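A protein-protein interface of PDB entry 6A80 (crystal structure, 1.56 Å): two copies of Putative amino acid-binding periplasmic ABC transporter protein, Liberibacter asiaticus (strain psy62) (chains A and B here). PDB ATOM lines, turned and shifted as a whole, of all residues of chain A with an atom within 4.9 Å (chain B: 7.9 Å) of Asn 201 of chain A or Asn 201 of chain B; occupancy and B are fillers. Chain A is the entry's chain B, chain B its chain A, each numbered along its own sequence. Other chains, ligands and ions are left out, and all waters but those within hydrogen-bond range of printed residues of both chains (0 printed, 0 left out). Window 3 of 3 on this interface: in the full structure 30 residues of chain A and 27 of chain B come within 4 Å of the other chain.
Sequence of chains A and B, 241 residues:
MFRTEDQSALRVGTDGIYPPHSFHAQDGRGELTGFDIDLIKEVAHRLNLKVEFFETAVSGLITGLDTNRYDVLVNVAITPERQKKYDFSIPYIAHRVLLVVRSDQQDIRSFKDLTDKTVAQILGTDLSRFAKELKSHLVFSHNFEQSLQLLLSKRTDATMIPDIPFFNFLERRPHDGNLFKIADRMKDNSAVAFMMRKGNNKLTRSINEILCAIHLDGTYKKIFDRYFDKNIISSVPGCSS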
ATOM      1  N   ASP A  87      14.656  -8.673   0.124  1.00  0.00           N
ATOM      2  CA  ASP A  87      14.365  -8.497   1.540  1.00  0.00           C
ATOM      3  C   ASP A  87      13.684  -9.821   2.020  1.00  0.00           C
ATOM      4  O   ASP A  87      12.819 -10.401   1.333  1.00  0.00           O
ATOM      5  CB  ASP A  87      13.392  -7.350   1.808  1.00  0.00           C
ATOM      6  CG  ASP A  87      14.052  -5.964   1.755  1.00  0.00           C
ATOM      7  OD1 ASP A  87      15.234  -5.872   1.467  1.00  0.00           O
ATOM      8  OD2 ASP A  87      13.344  -4.983   2.012  1.00  0.00           O
ATOM      9  N   GLY A 199      14.586  -3.272  -0.893  1.00  0.00           N
ATOM     10  CA  GLY A 199      14.061  -1.925  -0.750  1.00  0.00           C
ATOM     11  C   GLY A 199      12.579  -1.871  -0.386  1.00  0.00           C
ATOM     12  O   GLY A 199      12.043  -0.793  -0.136  1.00  0.00           O
ATOM     13  N   ASN A 200      11.895  -3.023  -0.337  1.00  0.00           N
ATOM     14  CA  ASN A 200      10.497  -3.029   0.106  1.00  0.00           C
ATOM     15  C   ASN A 200      10.455  -3.089   1.650  1.00  0.00           C
ATOM     16  O   ASN A 200       9.839  -3.994   2.241  1.00  0.00           O
ATOM     17  CB  ASN A 200       9.713  -4.154  -0.582  1.00  0.00           C
ATOM     18  CG  ASN A 200       8.274  -3.802  -0.804  1.00  0.00           C
ATOM     19  OD1 ASN A 200       7.684  -2.991  -0.061  1.00  0.00           O
ATOM     20  ND2 ASN A 200       7.667  -4.424  -1.808  1.00  0.00           N
ATOM     21  N   ASN A 201      11.137  -2.130   2.283  1.00  0.00           N
ATOM     22  CA  ASN A 201      11.489  -2.203   3.711  1.00  0.00           C
ATOM     23  C   ASN A 201      10.293  -1.925   4.603  1.00  0.00           C
ATOM     24  O   ASN A 201      10.212  -2.429   5.710  1.00  0.00           O
ATOM     25  CB  ASN A 201      12.654  -1.261   4.094  1.00  0.00           C
ATOM     26  CG  ASN A 201      13.894  -1.437   3.213  1.00  0.00           C
ATOM     27  OD1 ASN A 201      14.414  -2.543   3.020  1.00  0.00           O
ATOM     28  ND2 ASN A 201      14.364  -0.325   2.650  1.00  0.00           N
ATOM     29  N   LYS A 202       9.360  -1.099   4.144  1.00  0.00           N
ATOM     30  CA  LYS A 202       8.198  -0.836   4.950  1.00  0.00           C
ATOM     31  C   LYS A 202       7.225  -2.042   4.945  1.00  0.00           C
ATOM     32  O   LYS A 202       6.623  -2.342   6.000  1.00  0.00           O
ATOM     33  CB  LYS A 202       7.541   0.515   4.547  1.00  0.00           C
ATOM     34  CG  LYS A 202       6.222   0.459   3.773  1.00  0.00           C
ATOM     35  CD  LYS A 202       6.005   1.709   2.901  1.00  0.00           C
ATOM     36  CE  LYS A 202       6.387   1.463   1.439  1.00  0.00           C
ATOM     37  NZ  LYS A 202       6.727   2.691   0.655  1.00  0.00           N
ATOM     38  N   LEU A 203       7.085  -2.731   3.793  1.00  0.00           N
ATOM     39  CA  LEU A 203       6.272  -3.955   3.744  1.00  0.00           C
ATOM     40  C   LEU A 203       6.935  -5.014   4.692  1.00  0.00           C
ATOM     41  O   LEU A 203       6.233  -5.671   5.452  1.00  0.00           O
ATOM     42  CB  LEU A 203       6.068  -4.446   2.326  1.00  0.00           C
ATOM     43  CG  LEU A 203       5.250  -5.734   2.259  1.00  0.00           C
ATOM     44  CD1 LEU A 203       3.909  -5.619   2.962  1.00  0.00           C
ATOM     45  CD2 LEU A 203       5.130  -6.356   0.859  1.00  0.00           C
ATOM     46  N   THR A 204       8.260  -5.098   4.661  1.00  0.00           N
ATOM     47  CA  THR A 204       8.987  -6.155   5.444  1.00  0.00           C
ATOM     48  C   THR A 204       8.782  -5.861   6.922  1.00  0.00           C
ATOM     49  O   THR A 204       8.410  -6.748   7.716  1.00  0.00           O
ATOM     50  CB  THR A 204      10.466  -6.196   5.067  1.00  0.00           C
ATOM     51  OG1 THR A 204      10.565  -6.427   3.665  1.00  0.00           O
ATOM     52  CG2 THR A 204      11.216  -7.339   5.892  1.00  0.00           C
ATOM     53  N   ARG A 205       8.983  -4.609   7.321  1.00  0.00           N
ATOM     54  CA  ARG A 205       8.786  -4.257   8.719  1.00  0.00           C
ATOM     55  C   ARG A 205       7.353  -4.534   9.179  1.00  0.00           C
ATOM     56  O   ARG A 205       7.164  -5.055  10.296  1.00  0.00           O
ATOM     57  CB  ARG A 205       9.207  -2.796   8.968  1.00  0.00           C
ATOM     58  CG  ARG A 205      10.663  -2.560   8.595  1.00  0.00           C
ATOM     59  CD  ARG A 205      11.131  -1.103   8.732  1.00  0.00           C
ATOM     60  NE  ARG A 205      11.581  -0.776  10.081  1.00  0.00           N
ATOM     61  CZ  ARG A 205      10.789  -0.770  11.150  1.00  0.00           C
ATOM     62  NH1 ARG A 205       9.504  -1.054  11.023  1.00  0.00           N
ATOM     63  NH2 ARG A 205      11.273  -0.459  12.347  1.00  0.00           N
ATOM     64  N   ASP B  87      15.617  -1.459  13.950  1.00  0.00           N
ATOM     65  CA  ASP B  87      15.858  -2.528  12.979  1.00  0.00           C
ATOM     66  C   ASP B  87      16.493  -3.704  13.734  1.00  0.00           C
ATOM     67  O   ASP B  87      17.384  -3.476  14.600  1.00  0.00           O
ATOM     68  CB  ASP B  87      16.945  -2.094  12.001  1.00  0.00           C
ATOM     69  CG  ASP B  87      16.430  -1.386  10.736  1.00  0.00           C
ATOM     70  OD1 ASP B  87      15.280  -0.908  10.704  1.00  0.00           O
ATOM     71  OD2 ASP B  87      17.247  -1.278   9.780  1.00  0.00           O
ATOM     72  N   MET B 196      19.530  -2.325  15.915  1.00  0.00           N
ATOM     73  CA  MET B 196      20.103  -1.107  15.280  1.00  0.00           C
ATOM     74  C   MET B 196      19.014  -0.026  15.155  1.00  0.00           C
ATOM     75  O   MET B 196      17.820  -0.305  15.295  1.00  0.00           O
ATOM     76  CB  MET B 196      20.602  -1.484  13.872  1.00  0.00           C
ATOM     77  CG  MET B 196      21.914  -2.235  13.906  1.00  0.00           C
ATOM     78  SD  MET B 196      22.087  -3.389  12.557  1.00  0.00           S
ATOM     79  CE  MET B 196      20.750  -4.645  12.831  1.00  0.00           C
ATOM     80  N   ARG B 197      19.443   1.246  14.979  1.00  0.00           N
ATOM     81  CA  ARG B 197      18.478   2.311  14.620  1.00  0.00           C
ATOM     82  C   ARG B 197      17.813   1.991  13.268  1.00  0.00           C
ATOM     83  O   ARG B 197      18.463   1.407  12.355  1.00  0.00           O
ATOM     84  CB  ARG B 197      19.223   3.631  14.499  1.00  0.00           C
ATOM     85  CG  ARG B 197      19.757   4.191  15.810  1.00  0.00           C
ATOM     86  CD  ARG B 197      20.226   5.660  15.626  1.00  0.00           C
ATOM     87  NE  ARG B 197      21.325   5.613  14.715  1.00  0.00           N
ATOM     88  CZ  ARG B 197      22.563   5.183  15.015  1.00  0.00           C
ATOM     89  NH1 ARG B 197      22.927   4.807  16.273  1.00  0.00           N
ATOM     90  NH2 ARG B 197      23.485   5.131  14.050  1.00  0.00           N
ATOM     91  N   LYS B 198      16.536   2.364  13.121  1.00  0.00           N
ATOM     92  CA  LYS B 198      15.936   2.284  11.761  1.00  0.00           C
ATOM     93  C   LYS B 198      16.741   3.089  10.786  1.00  0.00           C
ATOM     94  O   LYS B 198      17.357   4.091  11.165  1.00  0.00           O
ATOM     95  CB  LYS B 198      14.540   2.866  11.718  1.00  0.00           C
ATOM     96  CG  LYS B 198      13.536   2.174  12.573  1.00  0.00           C
ATOM     97  CD  LYS B 198      12.114   2.240  11.996  1.00  0.00           C
ATOM     98  CE  LYS B 198      11.656   3.657  11.762  1.00  0.00           C
ATOM     99  NZ  LYS B 198      10.186   3.636  11.566  1.00  0.00           N
ATOM    100  N   GLY B 199      16.722   2.636   9.539  1.00  0.00           N
ATOM    101  CA  GLY B 199      17.198   3.394   8.433  1.00  0.00           C
ATOM    102  C   GLY B 199      18.545   3.040   7.891  1.00  0.00           C
ATOM    103  O   GLY B 199      19.081   3.780   7.074  1.00  0.00           O
ATOM    104  N   ASN B 200      19.144   1.964   8.362  1.00  0.00           N
ATOM    105  CA  ASN B 200      20.303   1.483   7.614  1.00  0.00           C
ATOM    106  C   ASN B 200      20.095   0.011   7.275  1.00  0.00           C
ATOM    107  O   ASN B 200      20.749  -0.918   7.816  1.00  0.00           O
ATOM    108  CB  ASN B 200      21.672   1.754   8.276  1.00  0.00           C
ATOM    109  CG  ASN B 200      22.848   1.500   7.306  1.00  0.00           C
ATOM    110  OD1 ASN B 200      22.647   1.147   6.140  1.00  0.00           O
ATOM    111  ND2 ASN B 200      24.071   1.722   7.773  1.00  0.00           N
ATOM    112  N   ASN B 201      19.161  -0.142   6.350  1.00  0.00           N
ATOM    113  CA  ASN B 201      18.773  -1.389   5.786  1.00  0.00           C
ATOM    114  C   ASN B 201      19.998  -2.093   5.265  1.00  0.00           C
ATOM    115  O   ASN B 201      20.144  -3.304   5.481  1.00  0.00           O
ATOM    116  CB  ASN B 201      17.734  -1.085   4.716  1.00  0.00           C
ATOM    117  CG  ASN B 201      16.521  -0.384   5.308  1.00  0.00           C
ATOM    118  OD1 ASN B 201      16.104  -0.696   6.428  1.00  0.00           O
ATOM    119  ND2 ASN B 201      15.986   0.607   4.598  1.00  0.00           N
ATOM    120  N   LYS B 202      20.896  -1.330   4.627  1.00  0.00           N
ATOM    121  CA  LYS B 202      22.140  -1.849   4.082  1.00  0.00           C
ATOM    122  C   LYS B 202      22.980  -2.590   5.142  1.00  0.00           C
ATOM    123  O   LYS B 202      23.379  -3.738   4.902  1.00  0.00           O
ATOM    124  CB  LYS B 202      22.949  -0.727   3.396  1.00  0.00           C
ATOM    125  CG  LYS B 202      23.838  -1.193   2.243  1.00  0.00           C
ATOM    126  CD  LYS B 202      23.971  -0.129   1.147  1.00  0.00           C
ATOM    127  CE  LYS B 202      24.809  -0.590  -0.039  1.00  0.00           C
ATOM    128  NZ  LYS B 202      24.086  -1.461  -1.019  1.00  0.00           N
ATOM    129  N   LEU B 203      23.211  -1.985   6.302  1.00  0.00           N
ATOM    130  CA  LEU B 203      24.012  -2.638   7.342  1.00  0.00           C
ATOM    131  C   LEU B 203      23.283  -3.914   7.808  1.00  0.00           C
ATOM    132  O   LEU B 203      23.906  -4.969   7.958  1.00  0.00           O
ATOM    133  CB  LEU B 203      24.248  -1.750   8.553  1.00  0.00           C
ATOM    134  CG  LEU B 203      24.993  -2.313   9.757  1.00  0.00           C
ATOM    135  CD1 LEU B 203      26.357  -2.933   9.435  1.00  0.00           C
ATOM    136  CD2 LEU B 203      25.128  -1.268  10.848  1.00  0.00           C
ATOM    137  N   THR B 204      21.972  -3.771   8.033  1.00  0.00           N
ATOM    138  CA  THR B 204      21.142  -4.925   8.518  1.00  0.00           C
ATOM    139  C   THR B 204      21.240  -6.091   7.516  1.00  0.00           C
ATOM    140  O   THR B 204      21.573  -7.228   7.927  1.00  0.00           O
ATOM    141  CB  THR B 204      19.673  -4.484   8.719  1.00  0.00           C
ATOM    142  OG1 THR B 204      19.653  -3.455   9.714  1.00  0.00           O
ATOM    143  CG2 THR B 204      18.798  -5.644   9.216  1.00  0.00           C
ATOM    144  N   ARG B 205      20.944  -5.852   6.231  1.00  0.00           N
ATOM    145  CA  ARG B 205      21.056  -6.923   5.222  1.00  0.00           C
ATOM    146  C   ARG B 205      22.500  -7.522   5.156  1.00  0.00           C
ATOM    147  O   ARG B 205      22.652  -8.736   4.986  1.00  0.00           O
ATOM    148  CB  ARG B 205      20.502  -6.498   3.823  1.00  0.00           C
ATOM    149  CG  ARG B 205      18.975  -6.292   3.712  1.00  0.00           C
ATOM    150  CD  ARG B 205      18.517  -6.035   2.244  1.00  0.00           C
ATOM    151  NE  ARG B 205      19.046  -4.763   1.771  1.00  0.00           N
ATOM    152  CZ  ARG B 205      18.382  -3.607   1.729  1.00  0.00           C
ATOM    153  NH1 ARG B 205      17.089  -3.535   2.045  1.00  0.00           N
ATOM    154  NH2 ARG B 205      19.013  -2.510   1.318  1.00  0.00           N
ATOM    155  N   SER B 206      23.540  -6.702   5.327  1.00  0.00           N
ATOM    156  CA  SER B 206      24.910  -7.168   5.357  1.00  0.00           C
ATOM    157  C   SER B 206      25.163  -8.106   6.552  1.00  0.00           C
ATOM    158  O   SER B 206      25.745  -9.154   6.385  1.00  0.00           O
ATOM    159  CB  SER B 206      25.881  -6.023   5.447  1.00  0.00           C
ATOM    160  OG  SER B 206      25.807  -5.333   4.209  1.00  0.00           O
ATOM    161  N   ILE B 207      24.712  -7.701   7.746  1.00  0.00           N
ATOM    162  CA  ILE B 207      24.910  -8.520   8.949  1.00  0.00           C
ATOM    163  C   ILE B 207      24.174  -9.849   8.716  1.00  0.00           C
ATOM    164  O   ILE B 207      24.732 -10.921   9.083  1.00  0.00           O
ATOM    165  CB  ILE B 207      24.395  -7.762  10.210  1.00  0.00           C
ATOM    166  CG1 ILE B 207      25.324  -6.557  10.558  1.00  0.00           C
ATOM    167  CG2 ILE B 207      24.188  -8.689  11.428  1.00  0.00           C
ATOM    168  CD1 ILE B 207      24.828  -5.751  11.768  1.00  0.00           C
ATOM    169  N   ASN B 208      22.956  -9.745   8.181  1.00  0.00           N
ATOM    170  CA  ASN B 208      22.152 -10.955   7.930  1.00  0.00           C
ATOM    171  C   ASN B 208      22.854 -11.929   7.014  1.00  0.00           C
ATOM    172  O   ASN B 208      22.922 -13.139   7.280  1.00  0.00           O
ATOM    173  CB  ASN B 208      20.743 -10.641   7.446  1.00  0.00           C
ATOM    174  CG  ASN B 208      19.911  -9.952   8.487  1.00  0.00           C
ATOM    175  OD1 ASN B 208      20.295  -9.930   9.658  1.00  0.00           O
ATOM    176  ND2 ASN B 208      18.752  -9.476   8.118  1.00  0.00           N
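The side-chain amide nitrogen of Asn 201 of chain B sits close to the side-chain amide nitrogen of Asn 201 of chain A (2.7 Å). The guanidinium group of Arg 205 of chain B is in hydrogen-bond range of the side-chain amide oxygen of Asn 201 of chain A, at 3.0 Å. NH1 of Arg 205 of chain B is in salt-bridge range of OD1 of Asp 87 of chain A (3.0 Å). The side-chain carboxylate (OD1) of Asp 87 of chain B lies within salt-bridge range of the guanidinium group (NE) of Arg 205 of chain A, at 3.8 Å.
N of Met 196 of chain B lies within hydrogen-bond range of O of Asp 87 of chain B, 2.8 Å away. The side-chain hydroxyl of Thr 204 of chain B sits at hydrogen-bond distance from the side-chain carboxylate of Asp 87 of chain B. OD2 of Asp 87 of chain A sits at hydrogen-bond distance from N of Asn 200 of chain A, 3.4 Å away. The side-chain amide oxygen of Asn 201 of chain A lies close to the side-chain carboxylate of Asp 87 of chain A.
Among the printed residues, pairs that only touch across the chains: Arg 205 of chain A with Lys 198 of chain B and Gly 199 of chain A with Arg 205 of chain B.
Of the printed residues of chain B, Asn 201 of chain A touches Asn 201 and Arg 205. Printed residues of chain B within 4 Å of Arg 205 of chain A: Asp 87 (3.8 Å) and Lys 198 (2.8 Å). Printed residues of chain A within 4 Å of Arg 205 of chain B: Asp 87, Gly 199 and Asn 201. Printed residues of chain A within 4 Å of Asp 87 of chain B: Arg 205. Of the printed residues of chain A, Lys 198 of chain B touches Arg 205. Leu 203 of chain B touches none of the printed residues of chain A. Thr 204 of chain A touches none of the printed residues of chain B. The nearest printed residue of chain B that does not touch Asn 201 of chain A is Lys 202 of chain B (6.8 Å). The nearest printed residue of chain A that does not touch Asn 201 of chain B is Arg 205 of chain A (5.5 Å).
Printed residues of chain B that touch a printed residue of chain A: Asp 87, Lys 198, Asn 201 and Arg 205. Among the printed residues, 6 pairs touch across the chains.
Asp 87 of chain A touches Arg 205 of chain B, and with the chains exchanged Arg 205 of chain A touches Asp 87 of chain B. Gly 199 of chain A touches Arg 205 of chain B, but with the chains exchanged Arg 205 of chain A does not touch Gly 199 of chain B (6.2 Å). Asn 201 of chain B touches its own counterpart, Asn 201 of chain A. Asn 201 of chain A touches Arg 205 of chain B, but with the chains exchanged Arg 205 of chain A does not touch Asn 201 of chain B (5.5 Å). Positions printed for both chains: 87, 199, 200, 201, 202, 203, 204 and 205. Of the 6 pairs that touch across the chains among the printed residues, 3 have their exchanged pair printed and touching as well.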
